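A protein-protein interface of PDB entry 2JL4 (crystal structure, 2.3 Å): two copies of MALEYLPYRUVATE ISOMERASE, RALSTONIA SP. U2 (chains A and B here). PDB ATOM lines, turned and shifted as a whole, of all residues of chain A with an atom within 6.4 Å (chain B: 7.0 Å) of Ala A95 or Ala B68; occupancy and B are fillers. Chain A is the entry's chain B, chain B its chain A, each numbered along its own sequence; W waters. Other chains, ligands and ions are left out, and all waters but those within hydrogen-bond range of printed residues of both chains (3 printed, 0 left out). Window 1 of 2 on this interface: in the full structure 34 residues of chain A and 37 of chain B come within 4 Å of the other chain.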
ATOM      1  N   ARG A  90      -2.574  12.598  15.507  1.00  0.00           N
ATOM      2  CA  ARG A  90      -2.216  11.232  15.884  1.00  0.00           C
ATOM      3  C   ARG A  90      -3.361  10.271  15.599  1.00  0.00           C
ATOM      4  O   ARG A  90      -3.146   9.222  14.990  1.00  0.00           O
ATOM      5  CB  ARG A  90      -1.790  11.135  17.355  1.00  0.00           C
ATOM      6  CG  ARG A  90      -0.313  10.812  17.557  1.00  0.00           C
ATOM      7  CD  ARG A  90       0.124  11.059  18.995  1.00  0.00           C
ATOM      8  NE  ARG A  90       1.298  11.939  19.056  1.00  0.00           N
ATOM      9  CZ  ARG A  90       2.554  11.541  19.263  1.00  0.00           C
ATOM     10  NH1 ARG A  90       2.841  10.260  19.449  1.00  0.00           N
ATOM     11  NH2 ARG A  90       3.528  12.440  19.288  1.00  0.00           N
ATOM     12  N   GLN A  91      -4.572  10.645  16.015  1.00  0.00           N
ATOM     13  CA  GLN A  91      -5.757   9.807  15.854  1.00  0.00           C
ATOM     14  C   GLN A  91      -6.047   9.525  14.382  1.00  0.00           C
ATOM     15  O   GLN A  91      -6.454   8.422  14.036  1.00  0.00           O
ATOM     16  CB  GLN A  91      -6.977  10.429  16.558  1.00  0.00           C
ATOM     17  CG  GLN A  91      -8.114   9.434  16.857  1.00  0.00           C
ATOM     18  CD  GLN A  91      -8.942   9.081  15.629  1.00  0.00           C
ATOM     19  OE1 GLN A  91      -8.995   9.838  14.656  1.00  0.00           O
ATOM     20  NE2 GLN A  91      -9.602   7.926  15.672  1.00  0.00           N
ATOM     21  N   ARG A  92      -5.816  10.513  13.524  1.00  0.00           N
ATOM     22  CA  ARG A  92      -6.130  10.373  12.104  1.00  0.00           C
ATOM     23  C   ARG A  92      -5.117   9.496  11.370  1.00  0.00           C
ATOM     24  O   ARG A  92      -5.505   8.633  10.579  1.00  0.00           O
ATOM     25  CB  ARG A  92      -6.238  11.743  11.441  1.00  0.00           C
ATOM     26  CG  ARG A  92      -7.410  12.564  11.939  1.00  0.00           C
ATOM     27  CD  ARG A  92      -7.206  14.015  11.591  1.00  0.00           C
ATOM     28  NE  ARG A  92      -7.191  14.197  10.145  1.00  0.00           N
ATOM     29  CZ  ARG A  92      -6.687  15.253   9.521  1.00  0.00           C
ATOM     30  NH1 ARG A  92      -6.140  16.252  10.205  1.00  0.00           N
ATOM     31  NH2 ARG A  92      -6.733  15.303   8.201  1.00  0.00           N
ATOM     32  N   VAL A  93      -3.830   9.720  11.644  1.00  0.00           N
ATOM     33  CA  VAL A  93      -2.763   8.867  11.130  1.00  0.00           C
ATOM     34  C   VAL A  93      -2.982   7.407  11.587  1.00  0.00           C
ATOM     35  O   VAL A  93      -2.933   6.479  10.775  1.00  0.00           O
ATOM     36  CB  VAL A  93      -1.364   9.401  11.540  1.00  0.00           C
ATOM     37  CG1 VAL A  93      -0.262   8.439  11.116  1.00  0.00           C
ATOM     38  CG2 VAL A  93      -1.115  10.784  10.916  1.00  0.00           C
ATOM     39  N   ARG A  94      -3.263   7.220  12.876  1.00  0.00           N
ATOM     40  CA  ARG A  94      -3.522   5.886  13.405  1.00  0.00           C
ATOM     41  C   ARG A  94      -4.750   5.219  12.782  1.00  0.00           C
ATOM     42  O   ARG A  94      -4.738   4.003  12.576  1.00  0.00           O
ATOM     43  CB  ARG A  94      -3.611   5.897  14.932  1.00  0.00           C
ATOM     44  CG  ARG A  94      -2.262   5.987  15.649  1.00  0.00           C
ATOM     45  CD  ARG A  94      -2.383   5.577  17.107  1.00  0.00           C
ATOM     46  NE  ARG A  94      -1.098   5.599  17.809  1.00  0.00           N
ATOM     47  CZ  ARG A  94      -0.791   6.422  18.812  1.00  0.00           C
ATOM     48  NH1 ARG A  94      -1.681   7.313  19.251  1.00  0.00           N
ATOM     49  NH2 ARG A  94       0.412   6.364  19.383  1.00  0.00           N
ATOM     50  N   ALA A  95      -5.782   6.004  12.454  1.00  0.00           N
ATOM     51  CA  ALA A  95      -6.997   5.475  11.818  1.00  0.00           C
ATOM     52  C   ALA A  95      -6.751   5.034  10.375  1.00  0.00           C
ATOM     53  O   ALA A  95      -7.242   3.985   9.943  1.00  0.00           O
ATOM     54  CB  ALA A  95      -8.137   6.494  11.876  1.00  0.00           C
ATOM     55  N   LEU A  96      -5.997   5.847   9.637  1.00  0.00           N
ATOM     56  CA  LEU A  96      -5.602   5.524   8.272  1.00  0.00           C
ATOM     57  C   LEU A  96      -4.753   4.262   8.244  1.00  0.00           C
ATOM     58  O   LEU A  96      -4.943   3.409   7.378  1.00  0.00           O
ATOM     59  CB  LEU A  96      -4.823   6.681   7.636  1.00  0.00           C
ATOM     60  CG  LEU A  96      -5.588   7.944   7.235  1.00  0.00           C
ATOM     61  CD1 LEU A  96      -4.604   9.078   7.001  1.00  0.00           C
ATOM     62  CD2 LEU A  96      -6.474   7.708   6.006  1.00  0.00           C
ATOM     63  N   ALA A  97      -3.815   4.157   9.184  1.00  0.00           N
ATOM     64  CA  ALA A  97      -3.007   2.948   9.337  1.00  0.00           C
ATOM     65  C   ALA A  97      -3.890   1.737   9.617  1.00  0.00           C
ATOM     66  O   ALA A  97      -3.703   0.680   9.015  1.00  0.00           O
ATOM     67  CB  ALA A  97      -1.957   3.114  10.449  1.00  0.00           C
ATOM     68  N   ALA A  98      -4.858   1.906  10.514  1.00  0.00           N
ATOM     69  CA  ALA A  98      -5.701   0.803  10.963  1.00  0.00           C
ATOM     70  C   ALA A  98      -6.695   0.322   9.895  1.00  0.00           C
ATOM     71  O   ALA A  98      -7.155  -0.818   9.936  1.00  0.00           O
ATOM     72  CB  ALA A  98      -6.428   1.185  12.287  1.00  0.00           C
ATOM     73  N   ILE A  99      -7.026   1.184   8.940  1.00  0.00           N
ATOM     74  CA  ILE A  99      -7.804   0.754   7.779  1.00  0.00           C
ATOM     75  C   ILE A  99      -7.040  -0.330   7.025  1.00  0.00           C
ATOM     76  O   ILE A  99      -7.622  -1.348   6.645  1.00  0.00           O
ATOM     77  CB  ILE A  99      -8.165   1.933   6.847  1.00  0.00           C
ATOM     78  CG1 ILE A  99      -9.247   2.808   7.507  1.00  0.00           C
ATOM     79  CG2 ILE A  99      -8.629   1.434   5.474  1.00  0.00           C
ATOM     80  CD1 ILE A  99      -9.315   4.221   6.966  1.00  0.00           C
ATOM     81  N   VAL A 100      -5.737  -0.124   6.828  1.00  0.00           N
ATOM     82  CA  VAL A 100      -4.904  -1.134   6.181  1.00  0.00           C
ATOM     83  C   VAL A 100      -4.624  -2.310   7.117  1.00  0.00           C
ATOM     84  O   VAL A 100      -4.838  -3.469   6.751  1.00  0.00           O
ATOM     85  CB  VAL A 100      -3.554  -0.541   5.661  1.00  0.00           C
ATOM     86  CG1 VAL A 100      -2.646  -1.658   5.123  1.00  0.00           C
ATOM     87  CG2 VAL A 100      -3.804   0.534   4.578  1.00  0.00           C
ATOM     88  N   TYR A 142     -10.092   5.032   2.452  1.00  0.00           N
ATOM     89  CA  TYR A 142      -8.794   5.699   2.542  1.00  0.00           C
ATOM     90  C   TYR A 142      -8.757   6.910   1.612  1.00  0.00           C
ATOM     91  O   TYR A 142      -8.453   8.015   2.050  1.00  0.00           O
ATOM     92  CB  TYR A 142      -7.668   4.715   2.174  1.00  0.00           C
ATOM     93  CG  TYR A 142      -6.318   5.050   2.759  1.00  0.00           C
ATOM     94  CD1 TYR A 142      -5.854   4.401   3.910  1.00  0.00           C
ATOM     95  CD2 TYR A 142      -5.490   6.009   2.160  1.00  0.00           C
ATOM     96  CE1 TYR A 142      -4.593   4.718   4.466  1.00  0.00           C
ATOM     97  CE2 TYR A 142      -4.239   6.332   2.711  1.00  0.00           C
ATOM     98  CZ  TYR A 142      -3.796   5.680   3.856  1.00  0.00           C
ATOM     99  OH  TYR A 142      -2.560   5.999   4.389  1.00  0.00           O
ATOM    100  N   LEU A 145     -10.837   9.814   2.654  1.00  0.00           N
ATOM    101  CA  LEU A 145     -10.240  10.556   3.764  1.00  0.00           C
ATOM    102  C   LEU A 145      -9.112  11.487   3.301  1.00  0.00           C
ATOM    103  O   LEU A 145      -8.952  12.597   3.832  1.00  0.00           O
ATOM    104  CB  LEU A 145      -9.765   9.612   4.872  1.00  0.00           C
ATOM    105  CG  LEU A 145     -10.850   8.892   5.692  1.00  0.00           C
ATOM    106  CD1 LEU A 145     -10.276   7.694   6.462  1.00  0.00           C
ATOM    107  CD2 LEU A 145     -11.584   9.827   6.644  1.00  0.00           C
ATOM    108  N   GLN B  50     -16.165   4.739   5.711  1.00  0.00           N
ATOM    109  CA  GLN B  50     -15.810   3.318   5.666  1.00  0.00           C
ATOM    110  C   GLN B  50     -17.032   2.420   5.911  1.00  0.00           C
ATOM    111  O   GLN B  50     -17.049   1.248   5.495  1.00  0.00           O
ATOM    112  CB  GLN B  50     -14.680   3.009   6.654  1.00  0.00           C
ATOM    113  CG  GLN B  50     -13.929   1.708   6.374  1.00  0.00           C
ATOM    114  CD  GLN B  50     -12.852   1.407   7.411  1.00  0.00           C
ATOM    115  OE1 GLN B  50     -12.738   2.090   8.425  1.00  0.00           O
ATOM    116  NE2 GLN B  50     -12.061   0.373   7.157  1.00  0.00           N
ATOM    117  N   LEU B  63     -14.834  10.497  14.948  1.00  0.00           N
ATOM    118  CA  LEU B  63     -13.676   9.628  14.956  1.00  0.00           C
ATOM    119  C   LEU B  63     -14.066   8.230  14.520  1.00  0.00           C
ATOM    120  O   LEU B  63     -15.113   7.713  14.932  1.00  0.00           O
ATOM    121  CB  LEU B  63     -13.084   9.559  16.362  1.00  0.00           C
ATOM    122  CG  LEU B  63     -12.682  10.865  17.040  1.00  0.00           C
ATOM    123  CD1 LEU B  63     -12.260  10.549  18.457  1.00  0.00           C
ATOM    124  CD2 LEU B  63     -11.553  11.553  16.273  1.00  0.00           C
ATOM    125  N   ILE B  64     -13.215   7.624  13.695  1.00  0.00           N
ATOM    126  CA  ILE B  64     -13.384   6.234  13.266  1.00  0.00           C
ATOM    127  C   ILE B  64     -12.121   5.430  13.611  1.00  0.00           C
ATOM    128  O   ILE B  64     -11.084   6.022  13.959  1.00  0.00           O
ATOM    129  CB  ILE B  64     -13.733   6.128  11.755  1.00  0.00           C
ATOM    130  CG1 ILE B  64     -12.566   6.642  10.886  1.00  0.00           C
ATOM    131  CG2 ILE B  64     -15.045   6.891  11.451  1.00  0.00           C
ATOM    132  CD1 ILE B  64     -12.497   6.026   9.485  1.00  0.00           C
ATOM    133  N   GLN B  65     -12.233   4.098  13.518  1.00  0.00           N
ATOM    134  CA  GLN B  65     -11.173   3.131  13.863  1.00  0.00           C
ATOM    135  C   GLN B  65     -10.941   2.990  15.365  1.00  0.00           C
ATOM    136  O   GLN B  65     -10.210   3.783  15.974  1.00  0.00           O
ATOM    137  CB  GLN B  65      -9.854   3.413  13.129  1.00  0.00           C
ATOM    138  CG  GLN B  65      -9.887   3.081  11.642  1.00  0.00           C
ATOM    139  CD  GLN B  65     -10.115   1.606  11.357  1.00  0.00           C
ATOM    140  OE1 GLN B  65      -9.670   0.724  12.103  1.00  0.00           O
ATOM    141  NE2 GLN B  65     -10.796   1.329  10.264  1.00  0.00           N
ATOM    142  N   SER B  66     -11.539   1.948  15.946  1.00  0.00           N
ATOM    143  CA  SER B  66     -11.476   1.724  17.390  1.00  0.00           C
ATOM    144  C   SER B  66     -10.054   1.665  17.968  1.00  0.00           C
ATOM    145  O   SER B  66      -9.837   2.188  19.053  1.00  0.00           O
ATOM    146  CB  SER B  66     -12.349   0.522  17.827  1.00  0.00           C
ATOM    147  OG  SER B  66     -11.739  -0.725  17.562  1.00  0.00           O
ATOM    148  N   PRO B  67      -9.083   1.046  17.256  1.00  0.00           N
ATOM    149  CA  PRO B  67      -7.710   1.054  17.790  1.00  0.00           C
ATOM    150  C   PRO B  67      -7.163   2.468  17.972  1.00  0.00           C
ATOM    151  O   PRO B  67      -6.543   2.750  18.997  1.00  0.00           O
ATOM    152  CB  PRO B  67      -6.906   0.327  16.711  1.00  0.00           C
ATOM    153  CG  PRO B  67      -7.890  -0.538  16.028  1.00  0.00           C
ATOM    154  CD  PRO B  67      -9.137   0.310  15.978  1.00  0.00           C
ATOM    155  N   ALA B  68      -7.419   3.333  16.988  1.00  0.00           N
ATOM    156  CA  ALA B  68      -7.002   4.729  17.001  1.00  0.00           C
ATOM    157  C   ALA B  68      -7.766   5.543  18.045  1.00  0.00           C
ATOM    158  O   ALA B  68      -7.176   6.391  18.729  1.00  0.00           O
ATOM    159  CB  ALA B  68      -7.190   5.349  15.608  1.00  0.00           C
ATOM    160  N   ILE B  69      -9.075   5.302  18.150  1.00  0.00           N
ATOM    161  CA  ILE B  69      -9.925   6.005  19.124  1.00  0.00           C
ATOM    162  C   ILE B  69      -9.466   5.697  20.547  1.00  0.00           C
ATOM    163  O   ILE B  69      -9.397   6.586  21.394  1.00  0.00           O
ATOM    164  CB  ILE B  69     -11.448   5.664  18.943  1.00  0.00           C
ATOM    165  CG1 ILE B  69     -11.948   6.156  17.573  1.00  0.00           C
ATOM    166  CG2 ILE B  69     -12.286   6.291  20.058  1.00  0.00           C
ATOM    167  CD1 ILE B  69     -13.260   5.560  17.113  1.00  0.00           C
ATOM    168  N   ILE B  70      -9.138   4.434  20.797  1.00  0.00           N
ATOM    169  CA  ILE B  70      -8.744   3.991  22.127  1.00  0.00           C
ATOM    170  C   ILE B  70      -7.376   4.571  22.504  1.00  0.00           C
ATOM    171  O   ILE B  70      -7.183   5.014  23.647  1.00  0.00           O
ATOM    172  CB  ILE B  70      -8.803   2.442  22.254  1.00  0.00           C
ATOM    173  CG1 ILE B  70     -10.259   1.978  22.107  1.00  0.00           C
ATOM    174  CG2 ILE B  70      -8.230   1.981  23.597  1.00  0.00           C
ATOM    175  CD1 ILE B  70     -10.463   0.480  21.958  1.00  0.00           C
ATOM    176  N   GLU B  71      -6.446   4.596  21.550  1.00  0.00           N
ATOM    177  CA  GLU B  71      -5.156   5.239  21.765  1.00  0.00           C
ATOM    178  C   GLU B  71      -5.364   6.730  22.040  1.00  0.00           C
ATOM    179  O   GLU B  71      -4.612   7.343  22.806  1.00  0.00           O
ATOM    180  CB  GLU B  71      -4.224   5.035  20.559  1.00  0.00           C
ATOM    181  CG  GLU B  71      -3.695   3.598  20.387  1.00  0.00           C
ATOM    182  CD  GLU B  71      -2.396   3.286  21.154  1.00  0.00           C
ATOM    183  OE1 GLU B  71      -1.787   4.189  21.771  1.00  0.00           O
ATOM    184  OE2 GLU B  71      -1.967   2.114  21.119  1.00  0.00           O
ATOM    185  N   TRP B  72      -6.384   7.295  21.393  1.00  0.00           N
ATOM    186  CA  TRP B  72      -6.789   8.686  21.579  1.00  0.00           C
ATOM    187  C   TRP B  72      -7.315   8.927  23.000  1.00  0.00           C
ATOM    188  O   TRP B  72      -6.947   9.931  23.632  1.00  0.00           O
ATOM    189  CB  TRP B  72      -7.858   9.054  20.543  1.00  0.00           C
ATOM    190  CG  TRP B  72      -8.381  10.450  20.641  1.00  0.00           C
ATOM    191  CD1 TRP B  72      -7.786  11.589  20.157  1.00  0.00           C
ATOM    192  CD2 TRP B  72      -9.618  10.862  21.221  1.00  0.00           C
ATOM    193  NE1 TRP B  72      -8.574  12.679  20.414  1.00  0.00           N
ATOM    194  CE2 TRP B  72      -9.701  12.267  21.073  1.00  0.00           C
ATOM    195  CE3 TRP B  72     -10.661  10.186  21.866  1.00  0.00           C
ATOM    196  CZ2 TRP B  72     -10.790  13.010  21.550  1.00  0.00           C
ATOM    197  CZ3 TRP B  72     -11.743  10.928  22.346  1.00  0.00           C
ATOM    198  CH2 TRP B  72     -11.797  12.325  22.180  1.00  0.00           C
ATOM    199  N   LEU B  73      -8.168   8.018  23.486  1.00  0.00           N
ATOM    200  CA  LEU B  73      -8.746   8.128  24.823  1.00  0.00           C
ATOM    201  C   LEU B  73      -7.675   8.044  25.908  1.00  0.00           C
ATOM    202  O   LEU B  73      -7.738   8.761  26.923  1.00  0.00           O
ATOM    203  CB  LEU B  73      -9.780   7.026  25.081  1.00  0.00           C
ATOM    204  CG  LEU B  73     -11.114   7.009  24.338  1.00  0.00           C
ATOM    205  CD1 LEU B  73     -11.828   5.696  24.624  1.00  0.00           C
ATOM    206  CD2 LEU B  73     -11.985   8.196  24.749  1.00  0.00           C
ATOM    207  N   TYR B 167      -9.575  -5.515  24.259  1.00  0.00           N
ATOM    208  CA  TYR B 167      -9.661  -6.293  23.026  1.00  0.00           C
ATOM    209  C   TYR B 167     -10.041  -7.749  23.312  1.00  0.00           C
ATOM    210  O   TYR B 167     -10.819  -8.352  22.574  1.00  0.00           O
ATOM    211  CB  TYR B 167      -8.313  -6.275  22.312  1.00  0.00           C
ATOM    212  CG  TYR B 167      -7.988  -5.017  21.537  1.00  0.00           C
ATOM    213  CD1 TYR B 167      -7.898  -5.044  20.146  1.00  0.00           C
ATOM    214  CD2 TYR B 167      -7.723  -3.813  22.190  1.00  0.00           C
ATOM    215  CE1 TYR B 167      -7.579  -3.897  19.426  1.00  0.00           C
ATOM    216  CE2 TYR B 167      -7.405  -2.663  21.478  1.00  0.00           C
ATOM    217  CZ  TYR B 167      -7.333  -2.713  20.100  1.00  0.00           C
ATOM    218  OH  TYR B 167      -6.999  -1.584  19.388  1.00  0.00           O
HETATM  219  O   HOH W   1      -1.557   8.734  21.863  1.00  0.00           O
HETATM  220  O   HOH W   2      -4.667   8.019  18.550  1.00  0.00           O
HETATM  221  O   HOH W   3     -10.857   9.159  12.769  1.00  0.00           O
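The backbone carbonyl oxygen (O) of Ile B64 is in hydrogen-bond range of the side-chain amide nitrogen (NE2) of Gln A91, 3.0 Å away.
NH2 of Arg A94 is in salt-bridge range of OE1 of Glu B71 (3.9 Å).
The side-chain amide oxygen (OE1) of Gln B50 lies within hydrogen-bond range of the side-chain amide nitrogen (NE2) of Gln B65 (2.8 Å).
Among the printed residues, pairs that only touch across the chains: Gln A91 with Leu B63, Gln A91 with Ala B68, Gln A91 with Ile B69, Gln A91 with Trp B72, Arg A94 with Ala B68, Ala A95 with Ile B64, Ala A95 with Gln B65, Ala A95 with Ala B68, Ala A98 with Gln B65, Ile A99 with Gln B50 and Ile A99 with Gln B65.
Of the printed residues of chain B, Gln A91 touches Leu B63, Ile B64, Ala B68, Ile B69 and Trp B72.
Of chain B, only Ile B64, Gln B65 and Ala B68 come within 4 Å of Ala A95.
Of the printed residues of chain B, Ile A99 touches Gln B50 and Gln B65.
Ala B68 touches three residues of chain A.
Printed residues of chain A within 4 Å of Trp B72: Gln A91 (3.7 Å).
The nearest residue of chain B that does not touch Ala A95 is Gln B50 (6.0 Å).
The nearest residue of chain A that does not touch Ala B68 is Ala A98 (5.3 Å).
Of the 13 printed residues of chain A, 5 touch a printed residue of chain B.
Printed residues of chain A that touch a printed residue of chain B: Gln A91, Arg A94, Ala A95, Ala A98 and Ile A99.
Along chain A the printed residues that touch a printed residue of chain B span positions 91 to 99.
No position is printed for both chains.
Of the 13 pairs that touch across the chains among the printed residues, none has its exchanged pair printed and touching as well.
Water W3 bridges the side-chain amide oxygen of Gln A91 (2.7 Å) and the backbone NH of Ile B64 (3.0 Å).
Water W1 lies within hydrogen-bond range of the guanidinium group of Arg A94 (3.0 Å) and the backbone carbonyl oxygen of Glu B71 (3.5 Å).
Water W2 lies within hydrogen-bond range of the backbone carbonyl oxygen (O) of Ala B68 (3.0 Å), the guanidinium group (NH1) of Arg A94 (3.1 Å) and the backbone NH (N) of Trp B72 (3.4 Å).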
